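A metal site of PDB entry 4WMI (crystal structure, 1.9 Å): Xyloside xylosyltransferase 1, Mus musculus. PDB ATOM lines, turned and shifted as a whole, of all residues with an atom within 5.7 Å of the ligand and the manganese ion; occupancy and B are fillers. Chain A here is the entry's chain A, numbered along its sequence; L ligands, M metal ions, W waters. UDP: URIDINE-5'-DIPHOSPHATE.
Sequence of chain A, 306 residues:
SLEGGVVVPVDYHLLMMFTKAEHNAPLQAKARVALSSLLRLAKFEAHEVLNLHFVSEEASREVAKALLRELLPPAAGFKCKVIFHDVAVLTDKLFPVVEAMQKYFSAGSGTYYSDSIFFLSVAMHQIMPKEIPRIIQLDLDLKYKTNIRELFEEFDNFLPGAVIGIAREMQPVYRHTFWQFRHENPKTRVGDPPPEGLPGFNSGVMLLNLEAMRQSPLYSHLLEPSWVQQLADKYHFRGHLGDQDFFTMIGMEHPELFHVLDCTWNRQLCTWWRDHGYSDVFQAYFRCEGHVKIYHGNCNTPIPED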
ATOM      1  N   MET A  16       0.173   5.771  20.650  1.00  0.00           N
ATOM      2  CA  MET A  16       0.502   5.465  22.038  1.00  0.00           C
ATOM      3  C   MET A  16       0.652   6.746  22.841  1.00  0.00           C
ATOM      4  O   MET A  16       1.294   7.710  22.392  1.00  0.00           O
ATOM      5  CB  MET A  16       1.785   4.645  22.118  1.00  0.00           C
ATOM      6  CG  MET A  16       1.660   3.310  21.378  1.00  0.00           C
ATOM      7  SD  MET A  16       3.174   2.410  21.065  1.00  0.00           S
ATOM      8  CE  MET A  16       2.690   1.406  19.648  1.00  0.00           C
ATOM      9  N   MET A  17       0.099   6.716  24.047  1.00  0.00           N
ATOM     10  CA  MET A  17       0.335   7.757  25.035  1.00  0.00           C
ATOM     11  C   MET A  17       1.702   7.565  25.674  1.00  0.00           C
ATOM     12  O   MET A  17       2.022   6.472  26.127  1.00  0.00           O
ATOM     13  CB  MET A  17      -0.714   7.682  26.137  1.00  0.00           C
ATOM     14  CG  MET A  17      -2.138   7.882  25.669  1.00  0.00           C
ATOM     15  SD  MET A  17      -2.376   9.592  25.154  1.00  0.00           S
ATOM     16  CE  MET A  17      -1.656  10.463  26.558  1.00  0.00           C
ATOM     17  N   PHE A  18       2.510   8.613  25.716  1.00  0.00           N
ATOM     18  CA  PHE A  18       3.823   8.530  26.361  1.00  0.00           C
ATOM     19  C   PHE A  18       4.149   9.852  27.013  1.00  0.00           C
ATOM     20  O   PHE A  18       4.800  10.710  26.417  1.00  0.00           O
ATOM     21  CB  PHE A  18       4.911   8.152  25.360  1.00  0.00           C
ATOM     22  CG  PHE A  18       6.231   7.761  25.985  1.00  0.00           C
ATOM     23  CD1 PHE A  18       6.301   6.679  26.864  1.00  0.00           C
ATOM     24  CD2 PHE A  18       7.388   8.477  25.709  1.00  0.00           C
ATOM     25  CE1 PHE A  18       7.524   6.307  27.439  1.00  0.00           C
ATOM     26  CE2 PHE A  18       8.608   8.114  26.272  1.00  0.00           C
ATOM     27  CZ  PHE A  18       8.676   7.018  27.133  1.00  0.00           C
ATOM     28  N   THR A  19       3.655  10.026  28.233  1.00  0.00           N
ATOM     29  CA  THR A  19       3.740  11.306  28.924  1.00  0.00           C
ATOM     30  C   THR A  19       4.411  11.126  30.276  1.00  0.00           C
ATOM     31  O   THR A  19       4.381  10.044  30.872  1.00  0.00           O
ATOM     32  CB  THR A  19       2.350  11.907  29.173  1.00  0.00           C
ATOM     33  OG1 THR A  19       1.582  10.957  29.927  1.00  0.00           O
ATOM     34  CG2 THR A  19       1.624  12.195  27.861  1.00  0.00           C
ATOM     35  N   LYS A  20       4.977  12.225  30.780  1.00  0.00           N
ATOM     36  CA  LYS A  20       5.639  12.246  32.084  1.00  0.00           C
ATOM     37  C   LYS A  20       6.674  11.122  32.201  1.00  0.00           C
ATOM     38  O   LYS A  20       6.830  10.508  33.254  1.00  0.00           O
ATOM     39  CB  LYS A  20       4.590  12.141  33.209  1.00  0.00           C
ATOM     40  CG  LYS A  20       3.383  13.047  33.065  1.00  0.00           C
ATOM     41  CD  LYS A  20       3.730  14.502  33.364  1.00  0.00           C
ATOM     42  CE  LYS A  20       2.495  15.395  33.363  1.00  0.00           C
ATOM     43  NZ  LYS A  20       1.513  14.962  34.402  1.00  0.00           N
ATOM     44  N   ASN A  24      10.969   8.611  34.914  1.00  0.00           N
ATOM     45  CA  ASN A  24       9.981   7.582  35.197  1.00  0.00           C
ATOM     46  C   ASN A  24      10.520   6.284  34.611  1.00  0.00           C
ATOM     47  O   ASN A  24      10.097   5.827  33.541  1.00  0.00           O
ATOM     48  CB  ASN A  24       8.603   7.935  34.614  1.00  0.00           C
ATOM     49  CG  ASN A  24       7.500   6.986  35.066  1.00  0.00           C
ATOM     50  OD1 ASN A  24       7.734   5.865  35.503  1.00  0.00           O
ATOM     51  ND2 ASN A  24       6.267   7.452  34.945  1.00  0.00           N
ATOM     52  N   LEU A  27       8.113   3.318  33.552  1.00  0.00           N
ATOM     53  CA  LEU A  27       7.420   3.581  32.288  1.00  0.00           C
ATOM     54  C   LEU A  27       8.324   3.412  31.068  1.00  0.00           C
ATOM     55  O   LEU A  27       7.912   2.848  30.059  1.00  0.00           O
ATOM     56  CB  LEU A  27       6.821   4.990  32.289  1.00  0.00           C
ATOM     57  CG  LEU A  27       6.031   5.438  31.047  1.00  0.00           C
ATOM     58  CD1 LEU A  27       4.801   4.570  30.841  1.00  0.00           C
ATOM     59  CD2 LEU A  27       5.602   6.885  31.209  1.00  0.00           C
ATOM     60  N   LYS A  30       8.746  -0.250  30.439  1.00  0.00           N
ATOM     61  CA  LYS A  30       7.519  -0.744  29.809  1.00  0.00           C
ATOM     62  C   LYS A  30       7.529  -0.418  28.319  1.00  0.00           C
ATOM     63  O   LYS A  30       7.327  -1.298  27.476  1.00  0.00           O
ATOM     64  CB  LYS A  30       6.292  -0.136  30.478  1.00  0.00           C
ATOM     65  CG  LYS A  30       6.015  -0.696  31.854  1.00  0.00           C
ATOM     66  CD  LYS A  30       4.831   0.036  32.465  1.00  0.00           C
ATOM     67  CE  LYS A  30       4.497  -0.524  33.833  1.00  0.00           C
ATOM     68  NZ  LYS A  30       3.384   0.240  34.448  1.00  0.00           N
ATOM     69  N   VAL A  55       1.739  10.540  21.822  1.00  0.00           N
ATOM     70  CA  VAL A  55       1.220  11.720  22.505  1.00  0.00           C
ATOM     71  C   VAL A  55       2.071  11.972  23.756  1.00  0.00           C
ATOM     72  O   VAL A  55       2.107  11.160  24.675  1.00  0.00           O
ATOM     73  CB  VAL A  55      -0.272  11.553  22.868  1.00  0.00           C
ATOM     74  CG1 VAL A  55      -0.810  12.843  23.483  1.00  0.00           C
ATOM     75  CG2 VAL A  55      -1.068  11.206  21.629  1.00  0.00           C
ATOM     76  N   PHE A 118      -7.095  11.531  28.998  1.00  0.00           N
ATOM     77  CA  PHE A 118      -7.510  10.133  29.177  1.00  0.00           C
ATOM     78  C   PHE A 118      -8.783   9.788  28.380  1.00  0.00           C
ATOM     79  O   PHE A 118      -9.198   8.647  28.340  1.00  0.00           O
ATOM     80  CB  PHE A 118      -7.622   9.774  30.666  1.00  0.00           C
ATOM     81  CG  PHE A 118      -6.339  10.016  31.415  1.00  0.00           C
ATOM     82  CD1 PHE A 118      -5.186   9.303  31.091  1.00  0.00           C
ATOM     83  CD2 PHE A 118      -6.271  10.997  32.409  1.00  0.00           C
ATOM     84  CE1 PHE A 118      -3.985   9.540  31.761  1.00  0.00           C
ATOM     85  CE2 PHE A 118      -5.082  11.222  33.088  1.00  0.00           C
ATOM     86  CZ  PHE A 118      -3.935  10.503  32.771  1.00  0.00           C
ATOM     87  N   LEU A 138      -2.790   1.908  21.516  1.00  0.00           N
ATOM     88  CA  LEU A 138      -2.173   0.835  22.311  1.00  0.00           C
ATOM     89  C   LEU A 138      -1.511   1.399  23.548  1.00  0.00           C
ATOM     90  O   LEU A 138      -0.851   2.445  23.495  1.00  0.00           O
ATOM     91  CB  LEU A 138      -1.132   0.091  21.466  1.00  0.00           C
ATOM     92  CG  LEU A 138      -1.671  -0.531  20.171  1.00  0.00           C
ATOM     93  CD1 LEU A 138      -0.613  -0.568  19.066  1.00  0.00           C
ATOM     94  CD2 LEU A 138      -2.220  -1.921  20.452  1.00  0.00           C
ATOM     95  N   ASP A 139      -1.673   0.674  24.660  1.00  0.00           N
ATOM     96  CA  ASP A 139      -0.944   0.973  25.900  1.00  0.00           C
ATOM     97  C   ASP A 139       0.542   0.653  25.680  1.00  0.00           C
ATOM     98  O   ASP A 139       0.902  -0.031  24.735  1.00  0.00           O
ATOM     99  CB  ASP A 139      -1.494   0.126  27.057  1.00  0.00           C
ATOM    100  CG  ASP A 139      -2.688   0.769  27.746  1.00  0.00           C
ATOM    101  OD1 ASP A 139      -3.244   1.750  27.201  1.00  0.00           O
ATOM    102  OD2 ASP A 139      -3.077   0.286  28.817  1.00  0.00           O
ATOM    103  N   LEU A 140       1.392   1.175  26.557  1.00  0.00           N
ATOM    104  CA  LEU A 140       2.812   0.873  26.490  1.00  0.00           C
ATOM    105  C   LEU A 140       3.271  -0.245  27.431  1.00  0.00           C
ATOM    106  O   LEU A 140       4.440  -0.618  27.453  1.00  0.00           O
ATOM    107  CB  LEU A 140       3.669   2.146  26.633  1.00  0.00           C
ATOM    108  CG  LEU A 140       3.814   2.928  25.301  1.00  0.00           C
ATOM    109  CD1 LEU A 140       4.418   4.299  25.514  1.00  0.00           C
ATOM    110  CD2 LEU A 140       4.649   2.171  24.265  1.00  0.00           C
ATOM    111  N   ASP A 141       2.341  -0.783  28.222  1.00  0.00           N
ATOM    112  CA  ASP A 141       2.663  -1.922  29.096  1.00  0.00           C
ATOM    113  C   ASP A 141       2.163  -3.231  28.469  1.00  0.00           C
ATOM    114  O   ASP A 141       1.550  -4.057  29.143  1.00  0.00           O
ATOM    115  CB  ASP A 141       2.073  -1.731  30.491  1.00  0.00           C
ATOM    116  CG  ASP A 141       0.562  -1.535  30.486  1.00  0.00           C
ATOM    117  OD1 ASP A 141       0.001  -1.110  29.459  1.00  0.00           O
ATOM    118  OD2 ASP A 141      -0.072  -1.764  31.527  1.00  0.00           O
ATOM    119  N   LEU A 142       2.431  -3.373  27.179  1.00  0.00           N
ATOM    120  CA  LEU A 142       2.066  -4.519  26.378  1.00  0.00           C
ATOM    121  C   LEU A 142       3.327  -5.257  25.980  1.00  0.00           C
ATOM    122  O   LEU A 142       4.427  -4.708  26.055  1.00  0.00           O
ATOM    123  CB  LEU A 142       1.312  -4.087  25.120  1.00  0.00           C
ATOM    124  CG  LEU A 142       0.016  -3.272  25.264  1.00  0.00           C
ATOM    125  CD1 LEU A 142      -0.568  -3.003  23.885  1.00  0.00           C
ATOM    126  CD2 LEU A 142      -0.972  -4.082  26.080  1.00  0.00           C
ATOM    127  N   GLY A 204      -6.690  -1.053  26.730  1.00  0.00           N
ATOM    128  CA  GLY A 204      -5.274  -1.218  26.343  1.00  0.00           C
ATOM    129  C   GLY A 204      -4.996  -1.406  24.862  1.00  0.00           C
ATOM    130  O   GLY A 204      -3.878  -1.140  24.393  1.00  0.00           O
ATOM    131  N   LEU A 241     -11.365   5.599  35.257  1.00  0.00           N
ATOM    132  CA  LEU A 241     -10.574   5.017  34.159  1.00  0.00           C
ATOM    133  C   LEU A 241     -10.777   5.634  32.775  1.00  0.00           C
ATOM    134  O   LEU A 241     -10.303   5.085  31.770  1.00  0.00           O
ATOM    135  CB  LEU A 241     -10.758   3.473  34.116  1.00  0.00           C
ATOM    136  CG  LEU A 241     -10.385   2.765  35.421  1.00  0.00           C
ATOM    137  CD1 LEU A 241     -10.512   1.238  35.330  1.00  0.00           C
ATOM    138  CD2 LEU A 241      -8.967   3.154  35.811  1.00  0.00           C
ATOM    139  N   HIS A 296      -0.851  -7.959  28.264  1.00  0.00           N
ATOM    140  CA  HIS A 296      -1.055  -6.644  28.834  1.00  0.00           C
ATOM    141  C   HIS A 296      -0.753  -6.691  30.314  1.00  0.00           C
ATOM    142  O   HIS A 296      -1.555  -7.190  31.124  1.00  0.00           O
ATOM    143  CB  HIS A 296      -2.501  -6.198  28.562  1.00  0.00           C
ATOM    144  CG  HIS A 296      -2.802  -4.764  28.968  1.00  0.00           C
ATOM    145  ND1 HIS A 296      -4.034  -4.217  28.826  1.00  0.00           N
ATOM    146  CD2 HIS A 296      -2.002  -3.778  29.535  1.00  0.00           C
ATOM    147  CE1 HIS A 296      -4.007  -2.942  29.275  1.00  0.00           C
ATOM    148  NE2 HIS A 296      -2.756  -2.672  29.699  1.00  0.00           N
ATOM    149  N   GLY A 297       0.414  -6.156  30.676  1.00  0.00           N
ATOM    150  CA  GLY A 297       0.862  -6.179  32.065  1.00  0.00           C
ATOM    151  C   GLY A 297       0.243  -5.028  32.811  1.00  0.00           C
ATOM    152  O   GLY A 297       0.969  -4.160  33.330  1.00  0.00           O
ATOM    153  N   ASN A 298      -1.095  -4.987  32.864  1.00  0.00           N
ATOM    154  CA  ASN A 298      -1.748  -3.892  33.584  1.00  0.00           C
ATOM    155  C   ASN A 298      -1.568  -3.932  35.102  1.00  0.00           C
ATOM    156  O   ASN A 298      -1.113  -4.925  35.670  1.00  0.00           O
ATOM    157  CB  ASN A 298      -3.208  -3.588  33.116  1.00  0.00           C
ATOM    158  CG  ASN A 298      -4.194  -4.760  33.298  1.00  0.00           C
ATOM    159  OD1 ASN A 298      -5.408  -4.529  33.443  1.00  0.00           O
ATOM    160  ND2 ASN A 298      -3.710  -5.976  33.214  1.00  0.00           N
ATOM    161  N   CYS A 299      -1.917  -2.823  35.729  1.00  0.00           N
ATOM    162  CA  CYS A 299      -1.626  -2.521  37.136  1.00  0.00           C
ATOM    163  C   CYS A 299      -0.190  -2.933  37.530  1.00  0.00           C
ATOM    164  O   CYS A 299       0.029  -3.605  38.549  1.00  0.00           O
ATOM    165  CB  CYS A 299      -2.713  -3.033  38.097  1.00  0.00           C
ATOM    166  SG  CYS A 299      -2.747  -4.814  38.468  1.00  0.00           S
ATOM    167  N   ASN A 300       0.759  -2.536  36.696  1.00  0.00           N
ATOM    168  CA  ASN A 300       2.187  -2.780  36.950  1.00  0.00           C
ATOM    169  C   ASN A 300       2.536  -4.256  37.135  1.00  0.00           C
ATOM    170  O   ASN A 300       3.452  -4.571  37.879  1.00  0.00           O
ATOM    171  CB  ASN A 300       2.634  -2.000  38.186  1.00  0.00           C
ATOM    172  CG  ASN A 300       2.392  -0.523  38.047  1.00  0.00           C
ATOM    173  OD1 ASN A 300       2.768   0.070  37.047  1.00  0.00           O
ATOM    174  ND2 ASN A 300       1.745   0.071  39.038  1.00  0.00           N
HETATM  175  N1  UDP L   1       0.775   6.473  30.506  1.00  0.00           N
HETATM  176  C2  UDP L   1       1.782   7.444  30.309  1.00  0.00           C
HETATM  177  N3  UDP L   1       2.312   8.100  31.350  1.00  0.00           N
HETATM  178  C4  UDP L   1       1.873   7.843  32.579  1.00  0.00           C
HETATM  179  C5  UDP L   1       0.880   6.889  32.830  1.00  0.00           C
HETATM  180  C6  UDP L   1       0.337   6.208  31.747  1.00  0.00           C
HETATM  181  O2  UDP L   1       2.163   7.684  29.144  1.00  0.00           O
HETATM  182  O4  UDP L   1       2.368   8.460  33.537  1.00  0.00           O
HETATM  183  C1' UDP L   1       0.214   5.802  29.318  1.00  0.00           C
HETATM  184  C2' UDP L   1       0.977   4.547  28.942  1.00  0.00           C
HETATM  185  O2' UDP L   1       0.870   4.382  27.521  1.00  0.00           O
HETATM  186  C3' UDP L   1       0.170   3.442  29.610  1.00  0.00           C
HETATM  187  C4' UDP L   1      -1.268   3.973  29.537  1.00  0.00           C
HETATM  188  O4' UDP L   1      -1.131   5.398  29.562  1.00  0.00           O
HETATM  189  O3' UDP L   1       0.362   2.192  28.948  1.00  0.00           O
HETATM  190  C5' UDP L   1      -2.172   3.574  30.702  1.00  0.00           C
HETATM  191  O5' UDP L   1      -1.407   3.434  31.904  1.00  0.00           O
HETATM  192  PA  UDP L   1      -0.954   1.971  32.374  1.00  0.00           P
HETATM  193  O1A UDP L   1      -0.857   1.141  31.115  1.00  0.00           O
HETATM  194  O2A UDP L   1       0.227   2.055  33.321  1.00  0.00           O
HETATM  195  O3A UDP L   1      -2.256   1.590  33.240  1.00  0.00           O
HETATM  196  PB  UDP L   1      -3.157   0.254  33.145  1.00  0.00           P
HETATM  197  O1B UDP L   1      -4.472   0.954  33.175  1.00  0.00           O
HETATM  198  O2B UDP L   1      -2.898  -0.491  34.431  1.00  0.00           O
HETATM  199  O3B UDP L   1      -2.904  -0.490  31.839  1.00  0.00           O
HETATM  200 MN    MN M   1      -1.959  -0.818  30.316  1.00  0.00          MN
HETATM  201  O   HOH W   1       0.802  -1.144  34.049  1.00  0.00           O
HETATM  202  O   HOH W   2      -1.170   4.483  25.014  1.00  0.00           O
HETATM  203  O   HOH W   3      -1.667   0.825  36.273  1.00  0.00           O
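Merely in contact with the ligand: Phe 18 (3.3 Å), Asn 298 (3.4 Å) and Leu 27 (3.5 Å).
Hydrophobic or aromatic side chains that line the ligand: Met 17, Leu 27, Leu 140 and His 296.
Of the 22 residues printed, 11 come within 4 Å of the ligand.
The nearest printed residue that does not touch the ligand is Asn 24 (4.3 Å).
O of His 296 sits at hydrogen-bond distance from ND2 of Asn 298 (3.2 Å).
O of Asp 141 lies within hydrogen-bond range of N of Gly 297 (2.8 Å).
N of Asp 139 is in hydrogen-bond range of O of Gly 204, 2.9 Å away.
The backbone NH of Phe 18 lies within hydrogen-bond range of the backbone carbonyl oxygen of Val 55, 2.8 Å away.
N of Leu 27 lies within hydrogen-bond range of OD1 of Asn 24 (3.2 Å).
The side-chain amide oxygen (OD1) of Asn 300 is in hydrogen-bond range of the side-chain amino group (NZ) of Lys 30, 2.7 Å away.
O2' of the ligand lies within hydrogen-bond range of O of Met 17 (2.8 Å).
N of Leu 140 sits at hydrogen-bond distance from O3' of the ligand, at 2.8 Å.
An oxygen (O2B) of the ligand is in hydrogen-bond range of the backbone NH (N) of Cys 299, at 2.8 Å.
N of Thr 19 sits at hydrogen-bond distance from O2 of the ligand (2.9 Å).
A nitrogen (N3) of the ligand sits at hydrogen-bond distance from the backbone carbonyl oxygen (O) of Thr 19 (2.9 Å).
OG1 of Thr 19 is in hydrogen-bond range of N3 of the ligand.
The side-chain amino group of Lys 30 lies within salt-bridge range of an oxygen (O2A) of the ligand, at 3.8 Å.
The manganese ion is bound by O3B of the ligand (1.8 Å), NE2 of His 296 (2.1 Å), OD1 of Asp 141 (2.2 Å), OD2 of Asp 139 (2.2 Å), O1A of the ligand (2.4 Å) and OD2 of Asp 141 (2.4 Å).
Three residues have an atom within 4 Å of the manganese ion: Asp 139, Asp 141 and His 296.
Water W2 lies within hydrogen-bond range of O of Leu 138 (2.6 Å), N of Met 17 (2.7 Å) and O2' of the ligand (3.2 Å).
Water W1 lies within hydrogen-bond range of NZ of Lys 30 (3.0 Å), N of Asn 300 (3.0 Å), O of Gly 297 (3.1 Å) and O2A of the ligand (3.3 Å).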
